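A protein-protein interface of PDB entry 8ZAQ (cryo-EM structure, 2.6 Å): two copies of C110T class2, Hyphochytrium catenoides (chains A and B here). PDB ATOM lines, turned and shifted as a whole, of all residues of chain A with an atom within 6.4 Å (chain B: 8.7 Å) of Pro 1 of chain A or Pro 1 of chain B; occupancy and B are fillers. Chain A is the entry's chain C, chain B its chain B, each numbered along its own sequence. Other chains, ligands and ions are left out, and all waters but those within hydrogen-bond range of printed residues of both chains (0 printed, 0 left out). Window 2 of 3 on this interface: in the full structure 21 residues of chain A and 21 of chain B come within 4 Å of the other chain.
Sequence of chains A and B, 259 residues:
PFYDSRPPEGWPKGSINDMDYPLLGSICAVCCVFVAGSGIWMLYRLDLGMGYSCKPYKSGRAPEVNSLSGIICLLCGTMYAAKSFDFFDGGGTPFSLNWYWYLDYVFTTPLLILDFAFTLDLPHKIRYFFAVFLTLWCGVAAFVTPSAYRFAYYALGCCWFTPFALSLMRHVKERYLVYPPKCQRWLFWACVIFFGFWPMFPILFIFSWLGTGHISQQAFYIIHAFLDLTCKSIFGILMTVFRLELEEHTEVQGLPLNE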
ATOM      1  N   PRO A   1      -4.772  -4.144 -30.710  1.00  0.00           N
ATOM      2  CA  PRO A   1      -5.397  -3.126 -31.554  1.00  0.00           C
ATOM      3  C   PRO A   1      -6.361  -3.723 -32.562  1.00  0.00           C
ATOM      4  O   PRO A   1      -6.895  -3.009 -33.411  1.00  0.00           O
ATOM      5  CB  PRO A   1      -4.206  -2.483 -32.273  1.00  0.00           C
ATOM      6  CG  PRO A   1      -2.972  -2.924 -31.519  1.00  0.00           C
ATOM      7  CD  PRO A   1      -3.389  -3.788 -30.368  1.00  0.00           C
ATOM      8  N   PHE A   2      -6.583  -5.026 -32.459  1.00  0.00           N
ATOM      9  CA  PHE A   2      -7.230  -5.764 -33.528  1.00  0.00           C
ATOM     10  C   PHE A   2      -8.716  -5.949 -33.252  1.00  0.00           C
ATOM     11  O   PHE A   2      -9.125  -6.270 -32.134  1.00  0.00           O
ATOM     12  CB  PHE A   2      -6.551  -7.119 -33.708  1.00  0.00           C
ATOM     13  CG  PHE A   2      -6.328  -7.501 -35.140  1.00  0.00           C
ATOM     14  CD1 PHE A   2      -7.216  -7.110 -36.122  1.00  0.00           C
ATOM     15  CD2 PHE A   2      -5.229  -8.251 -35.505  1.00  0.00           C
ATOM     16  CE1 PHE A   2      -7.013  -7.466 -37.434  1.00  0.00           C
ATOM     17  CE2 PHE A   2      -5.024  -8.606 -36.817  1.00  0.00           C
ATOM     18  CZ  PHE A   2      -5.918  -8.219 -37.777  1.00  0.00           C
ATOM     19  N   TYR A   3      -9.513  -5.735 -34.280  1.00  0.00           N
ATOM     20  CA  TYR A   3     -10.950  -5.969 -34.290  1.00  0.00           C
ATOM     21  C   TYR A   3     -11.362  -6.926 -35.396  1.00  0.00           C
ATOM     22  O   TYR A   3     -12.297  -7.708 -35.210  1.00  0.00           O
ATOM     23  CB  TYR A   3     -11.694  -4.619 -34.432  1.00  0.00           C
ATOM     24  CG  TYR A   3     -13.182  -4.719 -34.699  1.00  0.00           C
ATOM     25  CD1 TYR A   3     -14.098  -4.575 -33.667  1.00  0.00           C
ATOM     26  CD2 TYR A   3     -13.673  -4.909 -35.985  1.00  0.00           C
ATOM     27  CE1 TYR A   3     -15.453  -4.656 -33.900  1.00  0.00           C
ATOM     28  CE2 TYR A   3     -15.027  -4.991 -36.226  1.00  0.00           C
ATOM     29  CZ  TYR A   3     -15.913  -4.862 -35.181  1.00  0.00           C
ATOM     30  OH  TYR A   3     -17.265  -4.937 -35.420  1.00  0.00           O
ATOM     31  N   ASP A   4     -10.684  -6.887 -36.537  1.00  0.00           N
ATOM     32  CA  ASP A   4     -11.024  -7.732 -37.667  1.00  0.00           C
ATOM     33  C   ASP A   4     -10.407  -9.116 -37.509  1.00  0.00           C
ATOM     34  O   ASP A   4      -9.484  -9.334 -36.721  1.00  0.00           O
ATOM     35  CB  ASP A   4     -10.548  -7.100 -38.974  1.00  0.00           C
ATOM     36  CG  ASP A   4     -10.718  -5.597 -38.990  1.00  0.00           C
ATOM     37  OD1 ASP A   4      -9.935  -4.902 -38.309  1.00  0.00           O
ATOM     38  OD2 ASP A   4     -11.633  -5.109 -39.683  1.00  0.00           O
ATOM     39  N   PRO A  94      -4.693 -12.703 -34.714  1.00  0.00           N
ATOM     40  CA  PRO A  94      -4.774 -11.647 -33.693  1.00  0.00           C
ATOM     41  C   PRO A  94      -3.471 -10.889 -33.485  1.00  0.00           C
ATOM     42  O   PRO A  94      -3.485  -9.664 -33.339  1.00  0.00           O
ATOM     43  CB  PRO A  94      -5.171 -12.421 -32.432  1.00  0.00           C
ATOM     44  CG  PRO A  94      -5.937 -13.582 -32.936  1.00  0.00           C
ATOM     45  CD  PRO A  94      -5.429 -13.914 -34.315  1.00  0.00           C
ATOM     46  N   TYR A 100      -1.440  -3.983 -39.664  1.00  0.00           N
ATOM     47  CA  TYR A 100      -1.273  -2.538 -39.582  1.00  0.00           C
ATOM     48  C   TYR A 100       0.047  -2.174 -40.245  1.00  0.00           C
ATOM     49  O   TYR A 100       1.121  -2.436 -39.696  1.00  0.00           O
ATOM     50  CB  TYR A 100      -1.331  -2.073 -38.131  1.00  0.00           C
ATOM     51  CG  TYR A 100      -2.634  -2.430 -37.462  1.00  0.00           C
ATOM     52  CD1 TYR A 100      -3.808  -1.778 -37.804  1.00  0.00           C
ATOM     53  CD2 TYR A 100      -2.696  -3.432 -36.503  1.00  0.00           C
ATOM     54  CE1 TYR A 100      -5.002  -2.101 -37.206  1.00  0.00           C
ATOM     55  CE2 TYR A 100      -3.891  -3.764 -35.900  1.00  0.00           C
ATOM     56  CZ  TYR A 100      -5.041  -3.093 -36.256  1.00  0.00           C
ATOM     57  OH  TYR A 100      -6.237  -3.414 -35.662  1.00  0.00           O
ATOM     58  N   LEU A 103       3.350  -0.248 -38.779  1.00  0.00           N
ATOM     59  CA  LEU A 103       3.368  -0.392 -37.329  1.00  0.00           C
ATOM     60  C   LEU A 103       4.654  -1.063 -36.864  1.00  0.00           C
ATOM     61  O   LEU A 103       5.230  -0.669 -35.846  1.00  0.00           O
ATOM     62  CB  LEU A 103       2.147  -1.180 -36.858  1.00  0.00           C
ATOM     63  CG  LEU A 103       2.016  -1.349 -35.343  1.00  0.00           C
ATOM     64  CD1 LEU A 103       2.128  -0.006 -34.635  1.00  0.00           C
ATOM     65  CD2 LEU A 103       0.712  -2.038 -34.990  1.00  0.00           C
ATOM     66  N   PRO B   1      -6.341  -2.681 -27.066  1.00  0.00           N
ATOM     67  CA  PRO B   1      -6.153  -3.937 -27.790  1.00  0.00           C
ATOM     68  C   PRO B   1      -7.317  -4.891 -27.611  1.00  0.00           C
ATOM     69  O   PRO B   1      -7.267  -6.029 -28.077  1.00  0.00           O
ATOM     70  CB  PRO B   1      -4.884  -4.523 -27.159  1.00  0.00           C
ATOM     71  CG  PRO B   1      -4.240  -3.395 -26.385  1.00  0.00           C
ATOM     72  CD  PRO B   1      -5.067  -2.158 -26.552  1.00  0.00           C
ATOM     73  N   PHE B   2      -8.362  -4.421 -26.942  1.00  0.00           N
ATOM     74  CA  PHE B   2      -9.401  -5.310 -26.453  1.00  0.00           C
ATOM     75  C   PHE B   2     -10.591  -5.347 -27.400  1.00  0.00           C
ATOM     76  O   PHE B   2     -11.041  -4.316 -27.907  1.00  0.00           O
ATOM     77  CB  PHE B   2      -9.844  -4.874 -25.059  1.00  0.00           C
ATOM     78  CG  PHE B   2     -10.010  -6.007 -24.094  1.00  0.00           C
ATOM     79  CD1 PHE B   2     -10.455  -7.241 -24.523  1.00  0.00           C
ATOM     80  CD2 PHE B   2      -9.721  -5.839 -22.755  1.00  0.00           C
ATOM     81  CE1 PHE B   2     -10.615  -8.277 -23.636  1.00  0.00           C
ATOM     82  CE2 PHE B   2      -9.875  -6.877 -21.868  1.00  0.00           C
ATOM     83  CZ  PHE B   2     -10.329  -8.090 -22.308  1.00  0.00           C
ATOM     84  N   TYR B   3     -11.087  -6.544 -27.636  1.00  0.00           N
ATOM     85  CA  TYR B   3     -12.295  -6.820 -28.402  1.00  0.00           C
ATOM     86  C   TYR B   3     -13.311  -7.610 -27.596  1.00  0.00           C
ATOM     87  O   TYR B   3     -14.515  -7.412 -27.770  1.00  0.00           O
ATOM     88  CB  TYR B   3     -11.924  -7.579 -29.700  1.00  0.00           C
ATOM     89  CG  TYR B   3     -13.095  -8.157 -30.468  1.00  0.00           C
ATOM     90  CD1 TYR B   3     -13.648  -7.472 -31.539  1.00  0.00           C
ATOM     91  CD2 TYR B   3     -13.620  -9.404 -30.149  1.00  0.00           C
ATOM     92  CE1 TYR B   3     -14.708  -7.995 -32.248  1.00  0.00           C
ATOM     93  CE2 TYR B   3     -14.680  -9.932 -30.852  1.00  0.00           C
ATOM     94  CZ  TYR B   3     -15.219  -9.225 -31.902  1.00  0.00           C
ATOM     95  OH  TYR B   3     -16.274  -9.752 -32.608  1.00  0.00           O
ATOM     96  N   ASP B   4     -12.855  -8.491 -26.713  1.00  0.00           N
ATOM     97  CA  ASP B   4     -13.742  -9.328 -25.929  1.00  0.00           C
ATOM     98  C   ASP B   4     -14.225  -8.588 -24.687  1.00  0.00           C
ATOM     99  O   ASP B   4     -13.660  -7.574 -24.270  1.00  0.00           O
ATOM    100  CB  ASP B   4     -13.041 -10.623 -25.518  1.00  0.00           C
ATOM    101  CG  ASP B   4     -12.144 -11.169 -26.605  1.00  0.00           C
ATOM    102  OD1 ASP B   4     -11.035 -10.626 -26.791  1.00  0.00           O
ATOM    103  OD2 ASP B   4     -12.546 -12.142 -27.274  1.00  0.00           O
ATOM    104  N   PRO B  94     -12.344  -3.463 -19.871  1.00  0.00           N
ATOM    105  CA  PRO B  94     -11.601  -2.889 -21.002  1.00  0.00           C
ATOM    106  C   PRO B  94     -10.120  -2.679 -20.724  1.00  0.00           C
ATOM    107  O   PRO B  94      -9.282  -2.967 -21.582  1.00  0.00           O
ATOM    108  CB  PRO B  94     -12.314  -1.554 -21.237  1.00  0.00           C
ATOM    109  CG  PRO B  94     -13.700  -1.784 -20.781  1.00  0.00           C
ATOM    110  CD  PRO B  94     -13.669  -2.839 -19.707  1.00  0.00           C
ATOM    111  N   PHE B  95      -9.779  -2.186 -19.535  1.00  0.00           N
ATOM    112  CA  PHE B  95      -8.381  -2.044 -19.133  1.00  0.00           C
ATOM    113  C   PHE B  95      -8.032  -3.212 -18.218  1.00  0.00           C
ATOM    114  O   PHE B  95      -7.927  -3.083 -17.000  1.00  0.00           O
ATOM    115  CB  PHE B  95      -8.139  -0.701 -18.454  1.00  0.00           C
ATOM    116  CG  PHE B  95      -6.702  -0.274 -18.463  1.00  0.00           C
ATOM    117  CD1 PHE B  95      -6.202   0.496 -19.499  1.00  0.00           C
ATOM    118  CD2 PHE B  95      -5.847  -0.652 -17.441  1.00  0.00           C
ATOM    119  CE1 PHE B  95      -4.881   0.888 -19.511  1.00  0.00           C
ATOM    120  CE2 PHE B  95      -4.525  -0.261 -17.448  1.00  0.00           C
ATOM    121  CZ  PHE B  95      -4.041   0.509 -18.484  1.00  0.00           C
ATOM    122  N   SER B  96      -7.851  -4.375 -18.829  1.00  0.00           N
ATOM    123  CA  SER B  96      -7.497  -5.587 -18.107  1.00  0.00           C
ATOM    124  C   SER B  96      -6.005  -5.836 -18.274  1.00  0.00           C
ATOM    125  O   SER B  96      -5.537  -6.103 -19.385  1.00  0.00           O
ATOM    126  CB  SER B  96      -8.303  -6.781 -18.611  1.00  0.00           C
ATOM    127  OG  SER B  96      -8.044  -7.936 -17.835  1.00  0.00           O
ATOM    128  N   LEU B  97      -5.265  -5.742 -17.173  1.00  0.00           N
ATOM    129  CA  LEU B  97      -3.860  -6.112 -17.146  1.00  0.00           C
ATOM    130  C   LEU B  97      -3.673  -7.595 -16.879  1.00  0.00           C
ATOM    131  O   LEU B  97      -2.536  -8.065 -16.767  1.00  0.00           O
ATOM    132  CB  LEU B  97      -3.114  -5.276 -16.105  1.00  0.00           C
ATOM    133  CG  LEU B  97      -2.997  -3.788 -16.448  1.00  0.00           C
ATOM    134  CD1 LEU B  97      -2.041  -3.087 -15.507  1.00  0.00           C
ATOM    135  CD2 LEU B  97      -2.567  -3.595 -17.892  1.00  0.00           C
ATOM    136  N   TRP B  99      -5.770  -9.856 -18.865  1.00  0.00           N
ATOM    137  CA  TRP B  99      -6.253 -10.532 -20.063  1.00  0.00           C
ATOM    138  C   TRP B  99      -5.105 -11.044 -20.922  1.00  0.00           C
ATOM    139  O   TRP B  99      -4.954 -12.252 -21.130  1.00  0.00           O
ATOM    140  CB  TRP B  99      -7.136  -9.585 -20.872  1.00  0.00           C
ATOM    141  CG  TRP B  99      -7.936 -10.293 -21.907  1.00  0.00           C
ATOM    142  CD1 TRP B  99      -7.666 -10.370 -23.239  1.00  0.00           C
ATOM    143  CD2 TRP B  99      -9.139 -11.036 -21.696  1.00  0.00           C
ATOM    144  NE1 TRP B  99      -8.628 -11.112 -23.873  1.00  0.00           N
ATOM    145  CE2 TRP B  99      -9.546 -11.531 -22.948  1.00  0.00           C
ATOM    146  CE3 TRP B  99      -9.916 -11.324 -20.571  1.00  0.00           C
ATOM    147  CZ2 TRP B  99     -10.692 -12.301 -23.107  1.00  0.00           C
ATOM    148  CZ3 TRP B  99     -11.050 -12.087 -20.730  1.00  0.00           C
ATOM    149  CH2 TRP B  99     -11.428 -12.567 -21.988  1.00  0.00           C
ATOM    150  N   TYR B 100      -4.292 -10.132 -21.440  1.00  0.00           N
ATOM    151  CA  TYR B 100      -3.184 -10.493 -22.314  1.00  0.00           C
ATOM    152  C   TYR B 100      -2.008 -10.906 -21.443  1.00  0.00           C
ATOM    153  O   TYR B 100      -1.369 -10.063 -20.805  1.00  0.00           O
ATOM    154  CB  TYR B 100      -2.829  -9.332 -23.239  1.00  0.00           C
ATOM    155  CG  TYR B 100      -3.988  -8.913 -24.108  1.00  0.00           C
ATOM    156  CD1 TYR B 100      -4.418  -9.719 -25.150  1.00  0.00           C
ATOM    157  CD2 TYR B 100      -4.663  -7.723 -23.878  1.00  0.00           C
ATOM    158  CE1 TYR B 100      -5.478  -9.351 -25.943  1.00  0.00           C
ATOM    159  CE2 TYR B 100      -5.728  -7.347 -24.668  1.00  0.00           C
ATOM    160  CZ  TYR B 100      -6.131  -8.165 -25.701  1.00  0.00           C
ATOM    161  OH  TYR B 100      -7.188  -7.803 -26.496  1.00  0.00           O
ATOM    162  N   LEU B 103       1.805  -9.419 -21.192  1.00  0.00           N
ATOM    163  CA  LEU B 103       1.807  -8.042 -21.669  1.00  0.00           C
ATOM    164  C   LEU B 103       2.329  -7.095 -20.597  1.00  0.00           C
ATOM    165  O   LEU B 103       3.100  -6.178 -20.895  1.00  0.00           O
ATOM    166  CB  LEU B 103       0.404  -7.632 -22.111  1.00  0.00           C
ATOM    167  CG  LEU B 103       0.273  -6.230 -22.712  1.00  0.00           C
ATOM    168  CD1 LEU B 103       1.327  -6.004 -23.787  1.00  0.00           C
ATOM    169  CD2 LEU B 103      -1.122  -6.007 -23.264  1.00  0.00           C
ATOM    170  N   PHE B 107       6.771  -4.676 -19.648  1.00  0.00           N
ATOM    171  CA  PHE B 107       7.042  -3.389 -19.016  1.00  0.00           C
ATOM    172  C   PHE B 107       8.020  -3.536 -17.855  1.00  0.00           C
ATOM    173  O   PHE B 107       8.860  -2.660 -17.648  1.00  0.00           O
ATOM    174  CB  PHE B 107       5.736  -2.735 -18.564  1.00  0.00           C
ATOM    175  CG  PHE B 107       4.710  -2.619 -19.655  1.00  0.00           C
ATOM    176  CD1 PHE B 107       4.961  -1.848 -20.776  1.00  0.00           C
ATOM    177  CD2 PHE B 107       3.498  -3.278 -19.559  1.00  0.00           C
ATOM    178  CE1 PHE B 107       4.023  -1.740 -21.782  1.00  0.00           C
ATOM    179  CE2 PHE B 107       2.557  -3.171 -20.563  1.00  0.00           C
ATOM    180  CZ  PHE B 107       2.821  -2.402 -21.675  1.00  0.00           C
ATOM    181  N   TRP B 137       7.404 -10.467 -25.899  1.00  0.00           N
ATOM    182  CA  TRP B 137       6.457 -10.237 -26.980  1.00  0.00           C
ATOM    183  C   TRP B 137       6.116 -11.513 -27.737  1.00  0.00           C
ATOM    184  O   TRP B 137       4.969 -11.674 -28.165  1.00  0.00           O
ATOM    185  CB  TRP B 137       6.993  -9.173 -27.934  1.00  0.00           C
ATOM    186  CG  TRP B 137       6.609  -7.803 -27.496  1.00  0.00           C
ATOM    187  CD1 TRP B 137       7.442  -6.813 -27.082  1.00  0.00           C
ATOM    188  CD2 TRP B 137       5.280  -7.279 -27.394  1.00  0.00           C
ATOM    189  NE1 TRP B 137       6.720  -5.698 -26.743  1.00  0.00           N
ATOM    190  CE2 TRP B 137       5.388  -5.958 -26.925  1.00  0.00           C
ATOM    191  CE3 TRP B 137       4.010  -7.797 -27.662  1.00  0.00           C
ATOM    192  CZ2 TRP B 137       4.278  -5.147 -26.718  1.00  0.00           C
ATOM    193  CZ3 TRP B 137       2.910  -6.991 -27.456  1.00  0.00           C
ATOM    194  CH2 TRP B 137       3.051  -5.681 -26.988  1.00  0.00           C
ATOM    195  N   VAL B 140       3.515 -13.055 -25.545  1.00  0.00           N
ATOM    196  CA  VAL B 140       2.225 -12.397 -25.742  1.00  0.00           C
ATOM    197  C   VAL B 140       1.571 -12.883 -27.030  1.00  0.00           C
ATOM    198  O   VAL B 140       0.376 -13.209 -27.058  1.00  0.00           O
ATOM    199  CB  VAL B 140       2.406 -10.867 -25.745  1.00  0.00           C
ATOM    200  CG1 VAL B 140       1.108 -10.173 -26.136  1.00  0.00           C
ATOM    201  CG2 VAL B 140       2.889 -10.381 -24.396  1.00  0.00           C
ATOM    202  N   VAL B 144      -2.020 -14.919 -27.377  1.00  0.00           N
ATOM    203  CA  VAL B 144      -3.164 -14.405 -28.128  1.00  0.00           C
ATOM    204  C   VAL B 144      -3.467 -15.221 -29.379  1.00  0.00           C
ATOM    205  O   VAL B 144      -4.552 -15.060 -29.958  1.00  0.00           O
ATOM    206  CB  VAL B 144      -2.979 -12.921 -28.514  1.00  0.00           C
ATOM    207  CG1 VAL B 144      -2.783 -12.068 -27.275  1.00  0.00           C
ATOM    208  CG2 VAL B 144      -1.818 -12.758 -29.479  1.00  0.00           C
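Pro 1 of chain A touches Pro 1 of chain B.
Tyr 3 of chain B touches Phe 2 of chain A.
Tyr 3 of chain B touches Tyr 3 of chain A (CD1 to CD1, 3.6 Å).
Val 144 of chain B touches Pro 94 of chain A (O to CG, 3.6 Å).
Pro 1 of chain A touches one residue of chain B.
Of the printed residues of chain B, Phe 2 of chain A touches Tyr 3.
Of the printed residues of chain B, Tyr 3 of chain A touches Tyr 3.
Pro 1 of chain B touches one residue of chain A.
Printed residues of chain A within 4 Å of Tyr 3 of chain B: Phe 2 and Tyr 3.
Of the printed residues of chain A, Val 144 of chain B touches Pro 94 (3.6 Å).
The nearest residue of chain B that does not touch Pro 1 of chain A is Phe 2 of chain B (5.2 Å).
The nearest residue of chain A that does not touch Pro 1 of chain B is Phe 2 of chain A (4.5 Å).
The nearest printed residue of chain B that does not touch Pro 94 of chain A is Tyr 100 of chain B (7.2 Å).
Of the 7 printed residues of chain A, 4 touch a printed residue of chain B.
Printed residues of chain A that touch a printed residue of chain B: Pro 1, Phe 2, Tyr 3 and Pro 94.
Hydrophobic or aromatic side chains of chain A within 4 Å of the printed part of chain B: Pro 1, Tyr 3 and Pro 94.
Of the 15 printed residues of chain B, 3 touch a printed residue of chain A.
Printed residues of chain B that touch a printed residue of chain A: Pro 1, Tyr 3 and Val 144.
Among the printed residues, no Asp or Glu carboxylate lies within 4 Å of a Lys or Arg side-chain nitrogen of the other chain.
Pro 1 of chain B touches its own counterpart, Pro 1 of chain A.
Phe 2 of chain A touches Tyr 3 of chain B, but with the chains exchanged Tyr 3 of chain A does not touch Phe 2 of chain B (6.5 Å).
Tyr 3 of chain A touches its own counterpart, Tyr 3 of chain B.
Of the 4 pairs that touch across the chains among the printed residues, 2 have their exchanged pair printed and touching as well.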
